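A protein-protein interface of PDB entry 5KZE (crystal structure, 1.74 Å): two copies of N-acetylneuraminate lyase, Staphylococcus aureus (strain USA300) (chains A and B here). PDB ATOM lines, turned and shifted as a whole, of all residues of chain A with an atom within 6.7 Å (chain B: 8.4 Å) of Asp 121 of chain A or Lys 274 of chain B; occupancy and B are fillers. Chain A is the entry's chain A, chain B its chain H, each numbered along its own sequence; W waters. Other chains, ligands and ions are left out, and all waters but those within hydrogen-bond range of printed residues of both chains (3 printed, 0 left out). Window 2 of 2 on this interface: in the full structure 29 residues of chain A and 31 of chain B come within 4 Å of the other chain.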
ATOM      1  N   LEU A  86       4.763  26.137  22.247  1.00  0.00           N
ATOM      2  CA  LEU A  86       4.433  25.641  23.582  1.00  0.00           C
ATOM      3  C   LEU A  86       5.095  26.469  24.677  1.00  0.00           C
ATOM      4  O   LEU A  86       4.486  26.762  25.696  1.00  0.00           O
ATOM      5  CB  LEU A  86       4.835  24.172  23.713  1.00  0.00           C
ATOM      6  CG  LEU A  86       4.650  23.500  25.077  1.00  0.00           C
ATOM      7  CD1 LEU A  86       3.181  23.438  25.492  1.00  0.00           C
ATOM      8  CD2 LEU A  86       5.269  22.118  25.060  1.00  0.00           C
ATOM      9  N   PHE A 114      -0.110  16.878  14.151  1.00  0.00           N
ATOM     10  CA  PHE A 114       0.234  16.281  15.434  1.00  0.00           C
ATOM     11  C   PHE A 114      -0.579  15.020  15.703  1.00  0.00           C
ATOM     12  O   PHE A 114      -1.753  14.947  15.330  1.00  0.00           O
ATOM     13  CB  PHE A 114       0.015  17.280  16.570  1.00  0.00           C
ATOM     14  CG  PHE A 114       0.911  18.481  16.506  1.00  0.00           C
ATOM     15  CD1 PHE A 114       2.286  18.351  16.650  1.00  0.00           C
ATOM     16  CD2 PHE A 114       0.382  19.745  16.311  1.00  0.00           C
ATOM     17  CE1 PHE A 114       3.109  19.453  16.599  1.00  0.00           C
ATOM     18  CE2 PHE A 114       1.214  20.854  16.259  1.00  0.00           C
ATOM     19  CZ  PHE A 114       2.575  20.703  16.402  1.00  0.00           C
ATOM     20  N   THR A 115       0.040  14.034  16.350  1.00  0.00           N
ATOM     21  CA  THR A 115      -0.678  12.846  16.795  1.00  0.00           C
ATOM     22  C   THR A 115      -1.444  13.210  18.054  1.00  0.00           C
ATOM     23  O   THR A 115      -1.188  14.251  18.658  1.00  0.00           O
ATOM     24  CB  THR A 115       0.259  11.648  17.100  1.00  0.00           C
ATOM     25  OG1 THR A 115       1.030  11.930  18.270  1.00  0.00           O
ATOM     26  CG2 THR A 115       1.200  11.376  15.943  1.00  0.00           C
ATOM     27  N   PHE A 116      -2.381  12.368  18.467  1.00  0.00           N
ATOM     28  CA  PHE A 116      -3.087  12.680  19.698  1.00  0.00           C
ATOM     29  C   PHE A 116      -2.135  12.698  20.887  1.00  0.00           C
ATOM     30  O   PHE A 116      -2.297  13.503  21.808  1.00  0.00           O
ATOM     31  CB  PHE A 116      -4.221  11.705  19.979  1.00  0.00           C
ATOM     32  CG  PHE A 116      -4.929  12.022  21.251  1.00  0.00           C
ATOM     33  CD1 PHE A 116      -5.529  13.256  21.415  1.00  0.00           C
ATOM     34  CD2 PHE A 116      -4.941  11.127  22.304  1.00  0.00           C
ATOM     35  CE1 PHE A 116      -6.162  13.584  22.593  1.00  0.00           C
ATOM     36  CE2 PHE A 116      -5.573  11.451  23.488  1.00  0.00           C
ATOM     37  CZ  PHE A 116      -6.188  12.682  23.630  1.00  0.00           C
ATOM     38  N   GLU A 117      -1.150  11.805  20.857  1.00  0.00           N
ATOM     39  CA  GLU A 117      -0.143  11.711  21.904  1.00  0.00           C
ATOM     40  C   GLU A 117       0.566  13.044  22.071  1.00  0.00           C
ATOM     41  O   GLU A 117       0.764  13.521  23.182  1.00  0.00           O
ATOM     42  CB  GLU A 117       0.872  10.601  21.589  1.00  0.00           C
ATOM     43  CG  GLU A 117       0.274   9.194  21.573  1.00  0.00           C
ATOM     44  CD  GLU A 117       1.130   8.180  20.808  1.00  0.00           C
ATOM     45  OE1 GLU A 117       2.176   8.568  20.244  1.00  0.00           O
ATOM     46  OE2 GLU A 117       0.757   6.983  20.771  1.00  0.00           O
ATOM     47  N   GLU A 118       0.935  13.657  20.960  1.00  0.00           N
ATOM     48  CA  GLU A 118       1.553  14.982  21.002  1.00  0.00           C
ATOM     49  C   GLU A 118       0.588  16.087  21.444  1.00  0.00           C
ATOM     50  O   GLU A 118       0.980  17.008  22.161  1.00  0.00           O
ATOM     51  CB  GLU A 118       2.154  15.305  19.637  1.00  0.00           C
ATOM     52  CG  GLU A 118       3.248  14.327  19.263  1.00  0.00           C
ATOM     53  CD  GLU A 118       3.677  14.401  17.817  1.00  0.00           C
ATOM     54  OE1 GLU A 118       2.854  14.792  16.962  1.00  0.00           O
ATOM     55  OE2 GLU A 118       4.853  14.059  17.543  1.00  0.00           O
ATOM     56  N   ILE A 119      -0.674  16.002  21.030  1.00  0.00           N
ATOM     57  CA  ILE A 119      -1.670  16.977  21.467  1.00  0.00           C
ATOM     58  C   ILE A 119      -1.927  16.834  22.974  1.00  0.00           C
ATOM     59  O   ILE A 119      -2.039  17.822  23.693  1.00  0.00           O
ATOM     60  CB  ILE A 119      -2.989  16.828  20.667  1.00  0.00           C
ATOM     61  CG1 ILE A 119      -2.757  17.209  19.202  1.00  0.00           C
ATOM     62  CG2 ILE A 119      -4.076  17.718  21.243  1.00  0.00           C
ATOM     63  CD1 ILE A 119      -3.925  16.932  18.293  1.00  0.00           C
ATOM     64  N   ARG A 120      -1.994  15.590  23.446  1.00  0.00           N
ATOM     65  CA  ARG A 120      -2.180  15.293  24.866  1.00  0.00           C
ATOM     66  C   ARG A 120      -1.087  15.889  25.738  1.00  0.00           C
ATOM     67  O   ARG A 120      -1.359  16.595  26.696  1.00  0.00           O
ATOM     68  CB  ARG A 120      -2.224  13.781  25.083  1.00  0.00           C
ATOM     69  CG  ARG A 120      -2.490  13.369  26.519  1.00  0.00           C
ATOM     70  CD  ARG A 120      -2.001  11.963  26.750  1.00  0.00           C
ATOM     71  NE  ARG A 120      -0.607  11.854  26.344  1.00  0.00           N
ATOM     72  CZ  ARG A 120      -0.028  10.728  25.959  1.00  0.00           C
ATOM     73  NH1 ARG A 120      -0.726   9.602  25.932  1.00  0.00           N
ATOM     74  NH2 ARG A 120       1.247  10.733  25.607  1.00  0.00           N
ATOM     75  N   ASP A 121       0.162  15.607  25.409  1.00  0.00           N
ATOM     76  CA  ASP A 121       1.247  16.040  26.280  1.00  0.00           C
ATOM     77  C   ASP A 121       1.482  17.553  26.244  1.00  0.00           C
ATOM     78  O   ASP A 121       2.056  18.111  27.165  1.00  0.00           O
ATOM     79  CB  ASP A 121       2.511  15.255  25.946  1.00  0.00           C
ATOM     80  CG  ASP A 121       2.405  13.799  26.396  1.00  0.00           C
ATOM     81  OD1 ASP A 121       1.553  13.511  27.266  1.00  0.00           O
ATOM     82  OD2 ASP A 121       3.146  12.946  25.890  1.00  0.00           O
ATOM     83  N   TYR A 122       0.995  18.219  25.203  1.00  0.00           N
ATOM     84  CA  TYR A 122       0.944  19.685  25.165  1.00  0.00           C
ATOM     85  C   TYR A 122       0.034  20.248  26.263  1.00  0.00           C
ATOM     86  O   TYR A 122       0.410  21.187  26.953  1.00  0.00           O
ATOM     87  CB  TYR A 122       0.498  20.123  23.765  1.00  0.00           C
ATOM     88  CG  TYR A 122      -0.139  21.487  23.567  1.00  0.00           C
ATOM     89  CD1 TYR A 122      -1.496  21.679  23.786  1.00  0.00           C
ATOM     90  CD2 TYR A 122       0.595  22.556  23.054  1.00  0.00           C
ATOM     91  CE1 TYR A 122      -2.095  22.909  23.554  1.00  0.00           C
ATOM     92  CE2 TYR A 122      -0.003  23.795  22.815  1.00  0.00           C
ATOM     93  CZ  TYR A 122      -1.351  23.956  23.069  1.00  0.00           C
ATOM     94  OH  TYR A 122      -1.975  25.162  22.837  1.00  0.00           O
ATOM     95  N   TYR A 123      -1.148  19.665  26.446  1.00  0.00           N
ATOM     96  CA  TYR A 123      -2.011  20.069  27.556  1.00  0.00           C
ATOM     97  C   TYR A 123      -1.350  19.756  28.880  1.00  0.00           C
ATOM     98  O   TYR A 123      -1.335  20.591  29.787  1.00  0.00           O
ATOM     99  CB  TYR A 123      -3.383  19.387  27.479  1.00  0.00           C
ATOM    100  CG  TYR A 123      -4.233  19.986  26.388  1.00  0.00           C
ATOM    101  CD1 TYR A 123      -4.762  21.262  26.518  1.00  0.00           C
ATOM    102  CD2 TYR A 123      -4.459  19.302  25.204  1.00  0.00           C
ATOM    103  CE1 TYR A 123      -5.517  21.829  25.506  1.00  0.00           C
ATOM    104  CE2 TYR A 123      -5.214  19.860  24.188  1.00  0.00           C
ATOM    105  CZ  TYR A 123      -5.740  21.123  24.344  1.00  0.00           C
ATOM    106  OH  TYR A 123      -6.487  21.680  23.324  1.00  0.00           O
ATOM    107  N   PHE A 124      -0.798  18.552  28.979  1.00  0.00           N
ATOM    108  CA  PHE A 124      -0.172  18.114  30.217  1.00  0.00           C
ATOM    109  C   PHE A 124       1.032  19.000  30.554  1.00  0.00           C
ATOM    110  O   PHE A 124       1.229  19.355  31.717  1.00  0.00           O
ATOM    111  CB  PHE A 124       0.248  16.635  30.127  1.00  0.00           C
ATOM    112  CG  PHE A 124      -0.914  15.667  30.018  1.00  0.00           C
ATOM    113  CD1 PHE A 124      -2.219  16.108  30.115  1.00  0.00           C
ATOM    114  CD2 PHE A 124      -0.686  14.321  29.818  1.00  0.00           C
ATOM    115  CE1 PHE A 124      -3.279  15.219  30.010  1.00  0.00           C
ATOM    116  CE2 PHE A 124      -1.736  13.429  29.712  1.00  0.00           C
ATOM    117  CZ  PHE A 124      -3.030  13.876  29.807  1.00  0.00           C
ATOM    118  N   ASP A 125       1.815  19.378  29.545  1.00  0.00           N
ATOM    119  CA  ASP A 125       3.024  20.191  29.776  1.00  0.00           C
ATOM    120  C   ASP A 125       2.729  21.625  30.242  1.00  0.00           C
ATOM    121  O   ASP A 125       3.505  22.213  30.997  1.00  0.00           O
ATOM    122  CB  ASP A 125       3.889  20.244  28.512  1.00  0.00           C
ATOM    123  CG  ASP A 125       4.662  18.964  28.271  1.00  0.00           C
ATOM    124  OD1 ASP A 125       4.734  18.111  29.183  1.00  0.00           O
ATOM    125  OD2 ASP A 125       5.216  18.807  27.165  1.00  0.00           O
ATOM    126  N   ILE A 126       1.625  22.193  29.768  1.00  0.00           N
ATOM    127  CA  ILE A 126       1.176  23.496  30.234  1.00  0.00           C
ATOM    128  C   ILE A 126       0.672  23.402  31.680  1.00  0.00           C
ATOM    129  O   ILE A 126       1.042  24.208  32.524  1.00  0.00           O
ATOM    130  CB  ILE A 126       0.062  24.071  29.328  1.00  0.00           C
ATOM    131  CG1 ILE A 126       0.604  24.366  27.927  1.00  0.00           C
ATOM    132  CG2 ILE A 126      -0.529  25.338  29.938  1.00  0.00           C
ATOM    133  CD1 ILE A 126      -0.473  24.659  26.924  1.00  0.00           C
ATOM    134  N   LEU A 155      -7.954  12.552  28.292  1.00  0.00           N
ATOM    135  CA  LEU A 155      -7.678  13.938  28.685  1.00  0.00           C
ATOM    136  C   LEU A 155      -8.328  14.306  30.019  1.00  0.00           C
ATOM    137  O   LEU A 155      -7.703  14.922  30.887  1.00  0.00           O
ATOM    138  CB  LEU A 155      -8.160  14.913  27.602  1.00  0.00           C
ATOM    139  CG  LEU A 155      -7.310  15.086  26.346  1.00  0.00           C
ATOM    140  CD1 LEU A 155      -7.962  16.093  25.416  1.00  0.00           C
ATOM    141  CD2 LEU A 155      -5.897  15.532  26.718  1.00  0.00           C
ATOM    142  N   GLU B  51      10.264  23.362  11.287  1.00  0.00           N
ATOM    143  CA  GLU B  51       9.441  23.540  12.486  1.00  0.00           C
ATOM    144  C   GLU B  51       9.258  25.024  12.793  1.00  0.00           C
ATOM    145  O   GLU B  51       9.060  25.421  13.942  1.00  0.00           O
ATOM    146  CB  GLU B  51      10.046  22.778  13.676  1.00  0.00           C
ATOM    147  CG  GLU B  51      10.039  21.274  13.427  1.00  0.00           C
ATOM    148  CD  GLU B  51      10.863  20.469  14.412  1.00  0.00           C
ATOM    149  OE1 GLU B  51      11.870  19.860  13.989  1.00  0.00           O
ATOM    150  OE2 GLU B  51      10.491  20.410  15.598  1.00  0.00           O
ATOM    151  N   LEU B  54       6.565  26.590  15.028  1.00  0.00           N
ATOM    152  CA  LEU B  54       6.671  26.301  16.449  1.00  0.00           C
ATOM    153  C   LEU B  54       7.594  27.307  17.140  1.00  0.00           C
ATOM    154  O   LEU B  54       7.729  27.286  18.361  1.00  0.00           O
ATOM    155  CB  LEU B  54       7.186  24.881  16.669  1.00  0.00           C
ATOM    156  CG  LEU B  54       6.433  23.777  15.937  1.00  0.00           C
ATOM    157  CD1 LEU B  54       6.802  22.439  16.540  1.00  0.00           C
ATOM    158  CD2 LEU B  54       4.954  24.012  16.058  1.00  0.00           C
ATOM    159  N   MET B 249       6.804   6.988  10.098  1.00  0.00           N
ATOM    160  CA  MET B 249       7.523   6.987  11.357  1.00  0.00           C
ATOM    161  C   MET B 249       7.445   8.327  12.052  1.00  0.00           C
ATOM    162  O   MET B 249       7.712   8.420  13.237  1.00  0.00           O
ATOM    163  CB  MET B 249       8.993   6.615  11.134  1.00  0.00           C
ATOM    164  CG  MET B 249       9.210   5.221  10.593  1.00  0.00           C
ATOM    165  SD  MET B 249      10.953   4.841  10.360  1.00  0.00           S
ATOM    166  CE  MET B 249      10.833   3.078  10.073  1.00  0.00           C
ATOM    167  N   GLY B 250       7.080   9.369  11.316  1.00  0.00           N
ATOM    168  CA  GLY B 250       7.182  10.725  11.830  1.00  0.00           C
ATOM    169  C   GLY B 250       8.342  11.433  11.155  1.00  0.00           C
ATOM    170  O   GLY B 250       9.502  11.249  11.518  1.00  0.00           O
ATOM    171  N   ILE B 251       8.014  12.259  10.174  1.00  0.00           N
ATOM    172  CA  ILE B 251       8.984  12.675   9.175  1.00  0.00           C
ATOM    173  C   ILE B 251      10.111  13.568   9.701  1.00  0.00           C
ATOM    174  O   ILE B 251      11.271  13.317   9.388  1.00  0.00           O
ATOM    175  CB  ILE B 251       8.268  13.378   7.996  1.00  0.00           C
ATOM    176  CG1 ILE B 251       9.236  13.621   6.840  1.00  0.00           C
ATOM    177  CG2 ILE B 251       7.583  14.673   8.440  1.00  0.00           C
ATOM    178  CD1 ILE B 251       8.534  13.833   5.529  1.00  0.00           C
ATOM    179  N   TYR B 252       9.797  14.597  10.484  1.00  0.00           N
ATOM    180  CA  TYR B 252      10.841  15.536  10.918  1.00  0.00           C
ATOM    181  C   TYR B 252      11.878  14.878  11.826  1.00  0.00           C
ATOM    182  O   TYR B 252      13.070  14.958  11.540  1.00  0.00           O
ATOM    183  CB  TYR B 252      10.238  16.762  11.626  1.00  0.00           C
ATOM    184  CG  TYR B 252       9.310  17.561  10.748  1.00  0.00           C
ATOM    185  CD1 TYR B 252       9.375  17.450   9.364  1.00  0.00           C
ATOM    186  CD2 TYR B 252       8.354  18.410  11.296  1.00  0.00           C
ATOM    187  CE1 TYR B 252       8.520  18.165   8.547  1.00  0.00           C
ATOM    188  CE2 TYR B 252       7.492  19.132  10.487  1.00  0.00           C
ATOM    189  CZ  TYR B 252       7.583  18.999   9.109  1.00  0.00           C
ATOM    190  OH  TYR B 252       6.742  19.705   8.275  1.00  0.00           O
ATOM    191  N   PRO B 253      11.442  14.248  12.931  1.00  0.00           N
ATOM    192  CA  PRO B 253      12.431  13.530  13.748  1.00  0.00           C
ATOM    193  C   PRO B 253      13.112  12.343  13.042  1.00  0.00           C
ATOM    194  O   PRO B 253      14.267  12.026  13.347  1.00  0.00           O
ATOM    195  CB  PRO B 253      11.608  13.045  14.958  1.00  0.00           C
ATOM    196  CG  PRO B 253      10.184  13.245  14.605  1.00  0.00           C
ATOM    197  CD  PRO B 253      10.146  14.366  13.625  1.00  0.00           C
ATOM    198  N   THR B 254      12.416  11.689  12.120  1.00  0.00           N
ATOM    199  CA  THR B 254      13.013  10.562  11.408  1.00  0.00           C
ATOM    200  C   THR B 254      14.090  11.003  10.410  1.00  0.00           C
ATOM    201  O   THR B 254      15.157  10.393  10.343  1.00  0.00           O
ATOM    202  CB  THR B 254      11.940   9.740  10.687  1.00  0.00           C
ATOM    203  OG1 THR B 254      11.031   9.211  11.661  1.00  0.00           O
ATOM    204  CG2 THR B 254      12.565   8.593   9.909  1.00  0.00           C
ATOM    205  N   LEU B 268      16.882  17.214  18.737  1.00  0.00           N
ATOM    206  CA  LEU B 268      15.496  16.816  18.956  1.00  0.00           C
ATOM    207  C   LEU B 268      14.510  17.672  18.165  1.00  0.00           C
ATOM    208  O   LEU B 268      14.866  18.737  17.664  1.00  0.00           O
ATOM    209  CB  LEU B 268      15.157  16.909  20.450  1.00  0.00           C
ATOM    210  CG  LEU B 268      15.921  16.020  21.431  1.00  0.00           C
ATOM    211  CD1 LEU B 268      15.645  16.459  22.867  1.00  0.00           C
ATOM    212  CD2 LEU B 268      15.566  14.557  21.230  1.00  0.00           C
ATOM    213  N   PRO B 269      13.256  17.205  18.058  1.00  0.00           N
ATOM    214  CA  PRO B 269      12.148  18.043  17.586  1.00  0.00           C
ATOM    215  C   PRO B 269      11.746  19.053  18.652  1.00  0.00           C
ATOM    216  O   PRO B 269      12.048  18.846  19.829  1.00  0.00           O
ATOM    217  CB  PRO B 269      11.008  17.036  17.341  1.00  0.00           C
ATOM    218  CG  PRO B 269      11.656  15.678  17.368  1.00  0.00           C
ATOM    219  CD  PRO B 269      12.830  15.817  18.287  1.00  0.00           C
ATOM    220  N   LYS B 270      11.086  20.132  18.253  1.00  0.00           N
ATOM    221  CA  LYS B 270      10.516  21.056  19.220  1.00  0.00           C
ATOM    222  C   LYS B 270       9.138  20.548  19.639  1.00  0.00           C
ATOM    223  O   LYS B 270       8.313  20.229  18.789  1.00  0.00           O
ATOM    224  CB  LYS B 270      10.427  22.464  18.634  1.00  0.00           C
ATOM    225  CG  LYS B 270      10.046  23.541  19.635  1.00  0.00           C
ATOM    226  CD  LYS B 270      10.286  24.927  19.038  1.00  0.00           C
ATOM    227  CE  LYS B 270      10.170  26.030  20.085  1.00  0.00           C
ATOM    228  NZ  LYS B 270       8.763  26.224  20.534  1.00  0.00           N
ATOM    229  N   ARG B 271       8.910  20.434  20.947  1.00  0.00           N
ATOM    230  CA  ARG B 271       7.622  19.980  21.432  1.00  0.00           C
ATOM    231  C   ARG B 271       6.599  21.027  21.032  1.00  0.00           C
ATOM    232  O   ARG B 271       6.928  22.206  20.926  1.00  0.00           O
ATOM    233  CB  ARG B 271       7.649  19.748  22.947  1.00  0.00           C
ATOM    234  CG  ARG B 271       8.351  18.453  23.335  1.00  0.00           C
ATOM    235  CD  ARG B 271       8.486  18.279  24.825  1.00  0.00           C
ATOM    236  NE  ARG B 271       9.111  19.441  25.456  1.00  0.00           N
ATOM    237  CZ  ARG B 271      10.421  19.606  25.618  1.00  0.00           C
ATOM    238  NH1 ARG B 271      11.278  18.686  25.185  1.00  0.00           N
ATOM    239  NH2 ARG B 271      10.875  20.698  26.215  1.00  0.00           N
ATOM    240  N   PRO B 272       5.345  20.614  20.834  1.00  0.00           N
ATOM    241  CA  PRO B 272       4.736  19.303  21.124  1.00  0.00           C
ATOM    242  C   PRO B 272       5.157  18.097  20.243  1.00  0.00           C
ATOM    243  O   PRO B 272       4.690  16.988  20.508  1.00  0.00           O
ATOM    244  CB  PRO B 272       3.240  19.584  20.939  1.00  0.00           C
ATOM    245  CG  PRO B 272       3.176  20.769  20.049  1.00  0.00           C
ATOM    246  CD  PRO B 272       4.334  21.610  20.451  1.00  0.00           C
ATOM    247  N   PHE B 273       5.998  18.295  19.229  1.00  0.00           N
ATOM    248  CA  PHE B 273       6.562  17.162  18.503  1.00  0.00           C
ATOM    249  C   PHE B 273       7.397  16.293  19.454  1.00  0.00           C
ATOM    250  O   PHE B 273       8.277  16.788  20.153  1.00  0.00           O
ATOM    251  CB  PHE B 273       7.422  17.631  17.326  1.00  0.00           C
ATOM    252  CG  PHE B 273       6.640  17.946  16.066  1.00  0.00           C
ATOM    253  CD1 PHE B 273       5.619  17.108  15.620  1.00  0.00           C
ATOM    254  CD2 PHE B 273       6.939  19.072  15.324  1.00  0.00           C
ATOM    255  CE1 PHE B 273       4.916  17.396  14.454  1.00  0.00           C
ATOM    256  CE2 PHE B 273       6.246  19.361  14.166  1.00  0.00           C
ATOM    257  CZ  PHE B 273       5.233  18.518  13.731  1.00  0.00           C
ATOM    258  N   LYS B 274       7.102  14.998  19.481  1.00  0.00           N
ATOM    259  CA  LYS B 274       7.885  14.050  20.272  1.00  0.00           C
ATOM    260  C   LYS B 274       9.076  13.494  19.493  1.00  0.00           C
ATOM    261  O   LYS B 274       9.026  13.385  18.267  1.00  0.00           O
ATOM    262  CB  LYS B 274       7.001  12.899  20.737  1.00  0.00           C
ATOM    263  CG  LYS B 274       5.986  13.280  21.772  1.00  0.00           C
ATOM    264  CD  LYS B 274       4.966  12.183  21.932  1.00  0.00           C
ATOM    265  CE  LYS B 274       3.995  12.501  23.039  1.00  0.00           C
ATOM    266  NZ  LYS B 274       4.718  12.854  24.281  1.00  0.00           N
ATOM    267  N   PRO B 275      10.144  13.101  20.208  1.00  0.00           N
ATOM    268  CA  PRO B 275      11.328  12.548  19.540  1.00  0.00           C
ATOM    269  C   PRO B 275      10.996  11.302  18.723  1.00  0.00           C
ATOM    270  O   PRO B 275       9.892  10.758  18.824  1.00  0.00           O
ATOM    271  CB  PRO B 275      12.266  12.205  20.701  1.00  0.00           C
ATOM    272  CG  PRO B 275      11.717  12.924  21.894  1.00  0.00           C
ATOM    273  CD  PRO B 275      10.248  13.027  21.672  1.00  0.00           C
ATOM    274  N   PHE B 276      11.948  10.876  17.901  1.00  0.00           N
ATOM    275  CA  PHE B 276      11.824   9.639  17.145  1.00  0.00           C
ATOM    276  C   PHE B 276      11.447   8.502  18.099  1.00  0.00           C
ATOM    277  O   PHE B 276      11.987   8.403  19.195  1.00  0.00           O
ATOM    278  CB  PHE B 276      13.139   9.340  16.398  1.00  0.00           C
ATOM    279  CG  PHE B 276      13.133   8.046  15.614  1.00  0.00           C
ATOM    280  CD1 PHE B 276      12.474   7.953  14.397  1.00  0.00           C
ATOM    281  CD2 PHE B 276      13.821   6.929  16.081  1.00  0.00           C
ATOM    282  CE1 PHE B 276      12.482   6.776  13.674  1.00  0.00           C
ATOM    283  CE2 PHE B 276      13.829   5.747  15.357  1.00  0.00           C
ATOM    284  CZ  PHE B 276      13.158   5.670  14.156  1.00  0.00           C
ATOM    285  N   ASN B 277      10.484   7.686  17.692  1.00  0.00           N
ATOM    286  CA  ASN B 277      10.087   6.503  18.444  1.00  0.00           C
ATOM    287  C   ASN B 277      11.049   5.355  18.147  1.00  0.00           C
ATOM    288  O   ASN B 277      11.060   4.799  17.041  1.00  0.00           O
ATOM    289  CB  ASN B 277       8.643   6.109  18.100  1.00  0.00           C
ATOM    290  CG  ASN B 277       8.042   5.132  19.093  1.00  0.00           C
ATOM    291  OD1 ASN B 277       8.744   4.327  19.698  1.00  0.00           O
ATOM    292  ND2 ASN B 277       6.723   5.192  19.252  1.00  0.00           N
HETATM  293  O   HOH W   1       6.148  24.604  20.191  1.00  0.00           O
HETATM  294  O   HOH W   2       6.901  13.551  16.325  1.00  0.00           O
HETATM  295  O   HOH W   3       3.747  16.969  22.898  1.00  0.00           O
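No position is printed for both chains.
Of the 9 pairs that touch across the chains among the printed residues, none has its exchanged pair printed and touching as well.
Of the 15 printed residues of chain A, 6 touch a printed residue of chain B.
Hydrophobic or aromatic side chains of chain A within 4 Å of the printed part of chain B: Leu 86, Phe 114 and Tyr 122.
Of the 18 printed residues of chain B, 4 touch a printed residue of chain A.
Printed residues of chain B that touch a printed residue of chain A: Arg 271, Pro 272, Phe 273 and Lys 274.
The side-chain hydroxyl (OG1) of Thr 115 of chain A lies close to the backbone NH (N) of Glu 117 of chain A.
OE1 of Glu 118 of chain A sits at hydrogen-bond distance from N of Thr 115 of chain A (3.0 Å).
NE of Arg 120 of chain A is in salt-bridge range of OD1 of Asp 121 of chain A.
Among the printed residues, pairs that only touch across the chains: Glu 118 of chain A with Pro 272 of chain B, Glu 117 of chain A with Lys 274 of chain B, Phe 114 of chain A with Phe 273 of chain B, Glu 118 of chain A with Phe 273 of chain B, Phe 114 of chain A with Pro 272 of chain B, Leu 86 of chain A with Arg 271 of chain B and Tyr 122 of chain A with Pro 272 of chain B.
Water W2 bridges OE2 of Glu 118 of chain A (2.4 Å) and O of Lys 274 of chain B (2.9 Å).
Water W3 lies within hydrogen-bond range of the backbone carbonyl oxygen of Pro 272 of chain B (2.6 Å) and the backbone carbonyl oxygen of Glu 118 of chain A (2.9 Å).
Water W1 lies within hydrogen-bond range of O of Arg 271 of chain B, N of Leu 86 of chain A and NZ of Lys 270 of chain B.
The backbone NH of Lys 274 of chain B sits at hydrogen-bond distance from the side-chain carboxylate of Glu 118 of chain A, 3.1 Å away.
OD2 of Asp 121 of chain A sits close to NZ of Lys 274 of chain B.
Asp 121 of chain A touches one residue of chain B.
Lys 274 of chain B touches just these residues of chain A: Glu 117 (3.4 Å), Glu 118 (3.1 Å) and Asp 121 (2.3 Å).
Of the printed residues of chain A, Pro 272 of chain B touches Phe 114, Glu 118 and Tyr 122.
Of the printed residues of chain B, Glu 117 of chain A touches Lys 274 (3.4 Å).
Of the printed residues of chain B, Phe 114 of chain A touches Pro 272 and Phe 273.
Of the printed residues of chain B, Glu 118 of chain A touches Pro 272 (3.2 Å), Phe 273 (3.7 Å) and Lys 274 (3.1 Å).
Printed residues of chain A within 4 Å of Arg 271 of chain B: Leu 86 (3.97 Å).
Asp 125 of chain A touches none of the printed residues of chain B.
Leu 268 of chain B touches none of the printed residues of chain A.
The nearest residue of chain A that does not touch Lys 274 of chain B is Arg 120 of chain A (4.2 Å).
The nearest printed residue of chain B that does not touch Leu 86 of chain A is Pro 272 of chain B (4.2 Å).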
